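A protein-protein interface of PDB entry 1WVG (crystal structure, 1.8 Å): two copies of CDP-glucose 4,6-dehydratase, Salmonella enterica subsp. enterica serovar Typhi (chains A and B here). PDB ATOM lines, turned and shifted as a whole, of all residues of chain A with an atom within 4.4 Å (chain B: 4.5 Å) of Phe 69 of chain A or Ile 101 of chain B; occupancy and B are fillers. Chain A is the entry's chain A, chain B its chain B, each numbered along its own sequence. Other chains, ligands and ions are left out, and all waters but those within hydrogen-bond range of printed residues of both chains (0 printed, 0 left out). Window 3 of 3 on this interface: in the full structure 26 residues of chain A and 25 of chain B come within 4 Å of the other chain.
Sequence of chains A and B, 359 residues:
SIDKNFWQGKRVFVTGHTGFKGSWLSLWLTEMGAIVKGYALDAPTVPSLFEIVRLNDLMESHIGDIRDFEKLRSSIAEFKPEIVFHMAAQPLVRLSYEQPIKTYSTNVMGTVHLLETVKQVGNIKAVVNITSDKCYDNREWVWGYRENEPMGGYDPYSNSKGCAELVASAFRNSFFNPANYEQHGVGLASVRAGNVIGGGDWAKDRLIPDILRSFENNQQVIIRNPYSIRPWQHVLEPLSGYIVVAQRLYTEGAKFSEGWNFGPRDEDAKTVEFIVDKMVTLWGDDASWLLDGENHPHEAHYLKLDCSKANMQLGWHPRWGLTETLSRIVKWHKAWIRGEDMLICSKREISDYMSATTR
Of chain B, only Ile 101 (3.6 Å) comes within 4 Å of Phe 69 of chain A. Lys 71 of chain A touches none of the printed residues of chain B. Of the printed residues of chain B, Val 112 of chain A touches Ile 101. Printed residues of chain B within 4 Å of His 113 of chain A: Ile 101 (3.7 Å). Of the printed residues of chain A, Pro 100 of chain B touches Glu 116 (3.6 Å). Thr 103 of chain B touches none of the printed residues of chain A. The nearest printed residue of chain B that does not touch Phe 69 of chain A is Pro 100 of chain B (8.3 Å). The nearest printed residue of chain A that does not touch Ile 101 of chain B is Gln 120 of chain A (5.6 Å). The nearest printed residue of chain A that does not touch Ser 105 of chain B is Val 112 of chain A (6.4 Å).
No position is printed for both chains. Of the 8 pairs that touch across the chains among the printed residues, none has its exchanged pair printed and touching as well.
Among the printed residues, pairs that only touch across the chains: Phe 69 of chain A with Ile 101 of chain B, Met 109 of chain A with Ile 101 of chain B, Met 109 of chain A with Tyr 104 of chain B, Val 112 of chain A with Ile 101 of chain B, His 113 of chain A with Ile 101 of chain B, Glu 116 of chain A with Pro 100 of chain B and Glu 116 of chain A with Ile 101 of chain B.
The backbone carbonyl oxygen (O) of Met 109 of chain A lies close to a ring nitrogen (ND1) of His 113 of chain A, at 3.4 Å. OE2 of Glu 116 of chain A lies within hydrogen-bond range of NE2 of Gln 120 of chain A, 3.1 Å away. The backbone carbonyl oxygen (O) of Ile 101 of chain B lies within hydrogen-bond range of the side-chain hydroxyl (OG) of Ser 105 of chain B (2.7 Å). O of Lys 102 of chain B sits at hydrogen-bond distance from OG of Ser 105 of chain B (2.9 Å).
The side-chain sulfur of Met 109 of chain A lies close to the backbone NH of Ser 105 of chain B.
Hydrophobic or aromatic side chains of chain A within 4 Å of the printed part of chain B: Phe 69, Met 109, Val 112 and His 113. Hydrophobic or aromatic side chains of chain B within 4 Å of the printed part of chain A: Pro 100, Ile 101 and Tyr 104. Among the printed residues, no Asp or Glu carboxylate lies within 4 Å of a Lys or Arg side-chain nitrogen of the other chain.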
ATOM      1  N   ARG A  67     -20.439 -20.148  -7.414  1.00  0.00           N
ATOM      2  CA  ARG A  67     -19.559 -19.057  -7.110  1.00  0.00           C
ATOM      3  C   ARG A  67     -19.834 -17.812  -7.944  1.00  0.00           C
ATOM      4  O   ARG A  67     -19.236 -16.759  -7.736  1.00  0.00           O
ATOM      5  CB  ARG A  67     -18.120 -19.518  -7.227  1.00  0.00           C
ATOM      6  CG  ARG A  67     -17.830 -20.605  -6.204  1.00  0.00           C
ATOM      7  CD  ARG A  67     -16.518 -21.301  -6.490  1.00  0.00           C
ATOM      8  NE  ARG A  67     -16.661 -22.255  -7.565  1.00  0.00           N
ATOM      9  CZ  ARG A  67     -15.674 -22.963  -8.107  1.00  0.00           C
ATOM     10  NH1 ARG A  67     -14.410 -22.869  -7.684  1.00  0.00           N
ATOM     11  NH2 ARG A  67     -15.960 -23.801  -9.115  1.00  0.00           N
ATOM     12  N   ASP A  68     -20.736 -17.915  -8.909  1.00  0.00           N
ATOM     13  CA  ASP A  68     -21.031 -16.750  -9.714  1.00  0.00           C
ATOM     14  C   ASP A  68     -22.293 -16.158  -9.146  1.00  0.00           C
ATOM     15  O   ASP A  68     -23.406 -16.581  -9.499  1.00  0.00           O
ATOM     16  CB  ASP A  68     -21.212 -17.212 -11.188  1.00  0.00           C
ATOM     17  CG  ASP A  68     -19.983 -17.842 -11.825  1.00  0.00           C
ATOM     18  OD1 ASP A  68     -18.837 -17.541 -11.506  1.00  0.00           O
ATOM     19  OD2 ASP A  68     -20.266 -18.721 -12.771  1.00  0.00           O
ATOM     20  N   PHE A  69     -22.099 -15.208  -8.230  1.00  0.00           N
ATOM     21  CA  PHE A  69     -23.237 -14.591  -7.533  1.00  0.00           C
ATOM     22  C   PHE A  69     -24.353 -14.066  -8.403  1.00  0.00           C
ATOM     23  O   PHE A  69     -25.532 -14.383  -8.234  1.00  0.00           O
ATOM     24  CB  PHE A  69     -22.862 -13.519  -6.474  1.00  0.00           C
ATOM     25  CG  PHE A  69     -24.071 -12.920  -5.756  1.00  0.00           C
ATOM     26  CD1 PHE A  69     -24.949 -13.709  -5.006  1.00  0.00           C
ATOM     27  CD2 PHE A  69     -24.334 -11.548  -5.813  1.00  0.00           C
ATOM     28  CE1 PHE A  69     -26.045 -13.174  -4.325  1.00  0.00           C
ATOM     29  CE2 PHE A  69     -25.428 -10.993  -5.143  1.00  0.00           C
ATOM     30  CZ  PHE A  69     -26.285 -11.804  -4.396  1.00  0.00           C
ATOM     31  N   GLU A  70     -23.924 -13.178  -9.271  1.00  0.00           N
ATOM     32  CA  GLU A  70     -24.757 -12.495 -10.206  1.00  0.00           C
ATOM     33  C   GLU A  70     -25.580 -13.489 -11.024  1.00  0.00           C
ATOM     34  O   GLU A  70     -26.812 -13.388 -11.089  1.00  0.00           O
ATOM     35  CB  GLU A  70     -23.843 -11.553 -11.019  1.00  0.00           C
ATOM     36  CG  GLU A  70     -22.760 -10.851 -10.122  1.00  0.00           C
ATOM     37  CD  GLU A  70     -21.331 -11.384 -10.214  1.00  0.00           C
ATOM     38  OE1 GLU A  70     -21.041 -12.569 -10.175  1.00  0.00           O
ATOM     39  OE2 GLU A  70     -20.421 -10.422 -10.289  1.00  0.00           O
ATOM     40  N   LYS A  71     -24.894 -14.487 -11.581  1.00  0.00           N
ATOM     41  CA  LYS A  71     -25.594 -15.486 -12.339  1.00  0.00           C
ATOM     42  C   LYS A  71     -26.582 -16.230 -11.463  1.00  0.00           C
ATOM     43  O   LYS A  71     -27.713 -16.479 -11.878  1.00  0.00           O
ATOM     44  CB  LYS A  71     -24.632 -16.470 -12.959  1.00  0.00           C
ATOM     45  CG  LYS A  71     -24.047 -15.965 -14.263  1.00  0.00           C
ATOM     46  CD  LYS A  71     -23.584 -17.108 -15.158  1.00  0.00           C
ATOM     47  CE  LYS A  71     -23.269 -18.398 -14.403  1.00  0.00           C
ATOM     48  NZ  LYS A  71     -24.425 -19.318 -14.259  1.00  0.00           N
ATOM     49  N   LEU A  72     -26.147 -16.611 -10.248  1.00  0.00           N
ATOM     50  CA  LEU A  72     -27.018 -17.344  -9.323  1.00  0.00           C
ATOM     51  C   LEU A  72     -28.263 -16.562  -8.968  1.00  0.00           C
ATOM     52  O   LEU A  72     -29.395 -17.065  -9.040  1.00  0.00           O
ATOM     53  CB  LEU A  72     -26.258 -17.729  -8.032  1.00  0.00           C
ATOM     54  CG  LEU A  72     -27.112 -18.328  -6.892  1.00  0.00           C
ATOM     55  CD1 LEU A  72     -27.859 -19.591  -7.322  1.00  0.00           C
ATOM     56  CD2 LEU A  72     -26.174 -18.706  -5.743  1.00  0.00           C
ATOM     57  N   ARG A  73     -28.017 -15.319  -8.550  1.00  0.00           N
ATOM     58  CA  ARG A  73     -29.083 -14.399  -8.165  1.00  0.00           C
ATOM     59  C   ARG A  73     -30.198 -14.320  -9.234  1.00  0.00           C
ATOM     60  O   ARG A  73     -31.416 -14.446  -8.961  1.00  0.00           O
ATOM     61  CB  ARG A  73     -28.481 -13.009  -7.852  1.00  0.00           C
ATOM     62  CG  ARG A  73     -29.493 -12.130  -7.114  1.00  0.00           C
ATOM     63  CD  ARG A  73     -29.336 -10.656  -7.414  1.00  0.00           C
ATOM     64  NE  ARG A  73     -28.234 -10.440  -8.333  1.00  0.00           N
ATOM     65  CZ  ARG A  73     -27.330  -9.485  -8.158  1.00  0.00           C
ATOM     66  NH1 ARG A  73     -27.363  -8.656  -7.110  1.00  0.00           N
ATOM     67  NH2 ARG A  73     -26.351  -9.378  -9.053  1.00  0.00           N
ATOM     68  N   MET A 109     -18.491 -19.698   0.200  1.00  0.00           N
ATOM     69  CA  MET A 109     -19.007 -18.571  -0.579  1.00  0.00           C
ATOM     70  C   MET A 109     -20.230 -18.958  -1.362  1.00  0.00           C
ATOM     71  O   MET A 109     -21.121 -18.139  -1.593  1.00  0.00           O
ATOM     72  CB  MET A 109     -17.942 -17.982  -1.498  1.00  0.00           C
ATOM     73  CG  MET A 109     -16.735 -17.403  -0.772  1.00  0.00           C
ATOM     74  SD  MET A 109     -17.144 -16.267   0.575  1.00  0.00           S
ATOM     75  CE  MET A 109     -18.096 -14.985  -0.279  1.00  0.00           C
ATOM     76  N   VAL A 112     -22.926 -18.429   1.094  1.00  0.00           N
ATOM     77  CA  VAL A 112     -23.117 -17.006   1.246  1.00  0.00           C
ATOM     78  C   VAL A 112     -23.901 -16.445   0.064  1.00  0.00           C
ATOM     79  O   VAL A 112     -24.827 -15.620   0.242  1.00  0.00           O
ATOM     80  CB  VAL A 112     -21.778 -16.304   1.291  1.00  0.00           C
ATOM     81  CG1 VAL A 112     -21.963 -14.752   1.384  1.00  0.00           C
ATOM     82  CG2 VAL A 112     -20.968 -16.890   2.460  1.00  0.00           C
ATOM     83  N   HIS A 113     -23.476 -16.880  -1.136  1.00  0.00           N
ATOM     84  CA  HIS A 113     -24.129 -16.393  -2.337  1.00  0.00           C
ATOM     85  C   HIS A 113     -25.580 -16.767  -2.335  1.00  0.00           C
ATOM     86  O   HIS A 113     -26.492 -15.981  -2.606  1.00  0.00           O
ATOM     87  CB  HIS A 113     -23.498 -16.955  -3.620  1.00  0.00           C
ATOM     88  CG  HIS A 113     -22.158 -16.369  -3.799  1.00  0.00           C
ATOM     89  ND1 HIS A 113     -21.256 -16.881  -4.724  1.00  0.00           N
ATOM     90  CD2 HIS A 113     -21.572 -15.332  -3.138  1.00  0.00           C
ATOM     91  CE1 HIS A 113     -20.141 -16.140  -4.633  1.00  0.00           C
ATOM     92  NE2 HIS A 113     -20.305 -15.194  -3.689  1.00  0.00           N
ATOM     93  N   GLU A 116     -27.314 -14.715   0.308  1.00  0.00           N
ATOM     94  CA  GLU A 116     -27.442 -13.328  -0.069  1.00  0.00           C
ATOM     95  C   GLU A 116     -28.471 -13.219  -1.190  1.00  0.00           C
ATOM     96  O   GLU A 116     -29.279 -12.291  -1.209  1.00  0.00           O
ATOM     97  CB  GLU A 116     -26.122 -12.702  -0.531  1.00  0.00           C
ATOM     98  CG  GLU A 116     -26.299 -11.204  -0.859  1.00  0.00           C
ATOM     99  CD  GLU A 116     -26.853 -10.380   0.294  1.00  0.00           C
ATOM    100  OE1 GLU A 116     -27.080 -10.807   1.401  1.00  0.00           O
ATOM    101  OE2 GLU A 116     -27.046  -9.135   0.013  1.00  0.00           O
ATOM    102  N   THR A 117     -28.443 -14.174  -2.123  1.00  0.00           N
ATOM    103  CA  THR A 117     -29.400 -14.178  -3.247  1.00  0.00           C
ATOM    104  C   THR A 117     -30.845 -14.287  -2.760  1.00  0.00           C
ATOM    105  O   THR A 117     -31.774 -13.629  -3.237  1.00  0.00           O
ATOM    106  CB  THR A 117     -29.077 -15.313  -4.206  1.00  0.00           C
ATOM    107  N   GLN A 120     -31.850 -10.835  -1.311  1.00  0.00           N
ATOM    108  CA  GLN A 120     -32.199  -9.859  -2.318  1.00  0.00           C
ATOM    109  C   GLN A 120     -33.474 -10.213  -3.103  1.00  0.00           C
ATOM    110  O   GLN A 120     -34.297  -9.349  -3.381  1.00  0.00           O
ATOM    111  CB  GLN A 120     -31.029  -9.666  -3.271  1.00  0.00           C
ATOM    112  CG  GLN A 120     -29.780  -9.203  -2.537  1.00  0.00           C
ATOM    113  CD  GLN A 120     -28.638  -9.020  -3.527  1.00  0.00           C
ATOM    114  OE1 GLN A 120     -28.803  -9.110  -4.754  1.00  0.00           O
ATOM    115  NE2 GLN A 120     -27.460  -8.767  -3.001  1.00  0.00           N
ATOM    116  N   GLN B  99     -22.630  -5.347   3.131  1.00  0.00           N
ATOM    117  CA  GLN B  99     -21.719  -6.082   2.283  1.00  0.00           C
ATOM    118  C   GLN B  99     -21.316  -7.458   2.787  1.00  0.00           C
ATOM    119  O   GLN B  99     -20.139  -7.754   2.856  1.00  0.00           O
ATOM    120  CB  GLN B  99     -20.409  -5.298   2.102  1.00  0.00           C
ATOM    121  CG  GLN B  99     -20.580  -3.891   1.507  1.00  0.00           C
ATOM    122  CD  GLN B  99     -21.638  -3.866   0.432  1.00  0.00           C
ATOM    123  OE1 GLN B  99     -21.411  -4.311  -0.705  1.00  0.00           O
ATOM    124  NE2 GLN B  99     -22.806  -3.348   0.794  1.00  0.00           N
ATOM    125  N   PRO B 100     -22.253  -8.324   3.113  1.00  0.00           N
ATOM    126  CA  PRO B 100     -21.877  -9.642   3.610  1.00  0.00           C
ATOM    127  C   PRO B 100     -20.940 -10.410   2.699  1.00  0.00           C
ATOM    128  O   PRO B 100     -19.938 -10.964   3.141  1.00  0.00           O
ATOM    129  CB  PRO B 100     -23.169 -10.429   3.852  1.00  0.00           C
ATOM    130  CG  PRO B 100     -24.317  -9.550   3.374  1.00  0.00           C
ATOM    131  CD  PRO B 100     -23.730  -8.195   2.976  1.00  0.00           C
ATOM    132  N   ILE B 101     -21.228 -10.437   1.404  1.00  0.00           N
ATOM    133  CA  ILE B 101     -20.367 -11.172   0.477  1.00  0.00           C
ATOM    134  C   ILE B 101     -18.933 -10.703   0.517  1.00  0.00           C
ATOM    135  O   ILE B 101     -17.967 -11.479   0.507  1.00  0.00           O
ATOM    136  CB  ILE B 101     -20.865 -11.063  -0.973  1.00  0.00           C
ATOM    137  CG1 ILE B 101     -22.254 -11.707  -1.132  1.00  0.00           C
ATOM    138  CG2 ILE B 101     -19.810 -11.650  -1.921  1.00  0.00           C
ATOM    139  CD1 ILE B 101     -22.751 -11.819  -2.577  1.00  0.00           C
ATOM    140  N   LYS B 102     -18.825  -9.388   0.533  1.00  0.00           N
ATOM    141  CA  LYS B 102     -17.540  -8.755   0.558  1.00  0.00           C
ATOM    142  C   LYS B 102     -16.770  -9.157   1.805  1.00  0.00           C
ATOM    143  O   LYS B 102     -15.576  -9.496   1.758  1.00  0.00           O
ATOM    144  CB  LYS B 102     -17.718  -7.240   0.424  1.00  0.00           C
ATOM    145  CG  LYS B 102     -16.448  -6.414   0.602  1.00  0.00           C
ATOM    146  CD  LYS B 102     -16.586  -4.991   0.069  1.00  0.00           C
ATOM    147  CE  LYS B 102     -15.914  -4.767  -1.276  1.00  0.00           C
ATOM    148  NZ  LYS B 102     -14.528  -4.225  -1.135  1.00  0.00           N
ATOM    149  N   THR B 103     -17.476  -9.086   2.924  1.00  0.00           N
ATOM    150  CA  THR B 103     -16.884  -9.414   4.212  1.00  0.00           C
ATOM    151  C   THR B 103     -16.336 -10.859   4.251  1.00  0.00           C
ATOM    152  O   THR B 103     -15.188 -11.160   4.644  1.00  0.00           O
ATOM    153  CB  THR B 103     -17.941  -9.142   5.303  1.00  0.00           C
ATOM    154  OG1 THR B 103     -18.315  -7.780   5.256  1.00  0.00           O
ATOM    155  CG2 THR B 103     -17.400  -9.438   6.693  1.00  0.00           C
ATOM    156  N   TYR B 104     -17.189 -11.774   3.814  1.00  0.00           N
ATOM    157  CA  TYR B 104     -16.815 -13.163   3.827  1.00  0.00           C
ATOM    158  C   TYR B 104     -15.705 -13.506   2.863  1.00  0.00           C
ATOM    159  O   TYR B 104     -14.742 -14.224   3.174  1.00  0.00           O
ATOM    160  CB  TYR B 104     -18.050 -14.077   3.638  1.00  0.00           C
ATOM    161  CG  TYR B 104     -18.931 -14.294   4.893  1.00  0.00           C
ATOM    162  CD1 TYR B 104     -20.180 -13.682   5.017  1.00  0.00           C
ATOM    163  CD2 TYR B 104     -18.551 -15.162   5.926  1.00  0.00           C
ATOM    164  CE1 TYR B 104     -21.010 -13.893   6.119  1.00  0.00           C
ATOM    165  CE2 TYR B 104     -19.356 -15.387   7.045  1.00  0.00           C
ATOM    166  CZ  TYR B 104     -20.590 -14.739   7.151  1.00  0.00           C
ATOM    167  OH  TYR B 104     -21.416 -14.989   8.237  1.00  0.00           O
ATOM    168  N   SER B 105     -15.840 -13.011   1.653  1.00  0.00           N
ATOM    169  CA  SER B 105     -14.837 -13.378   0.693  1.00  0.00           C
ATOM    170  C   SER B 105     -13.510 -12.875   1.123  1.00  0.00           C
ATOM    171  O   SER B 105     -12.487 -13.555   1.018  1.00  0.00           O
ATOM    172  CB  SER B 105     -15.191 -12.792  -0.640  1.00  0.00           C
ATOM    173  OG  SER B 105     -15.450 -11.449  -0.357  1.00  0.00           O
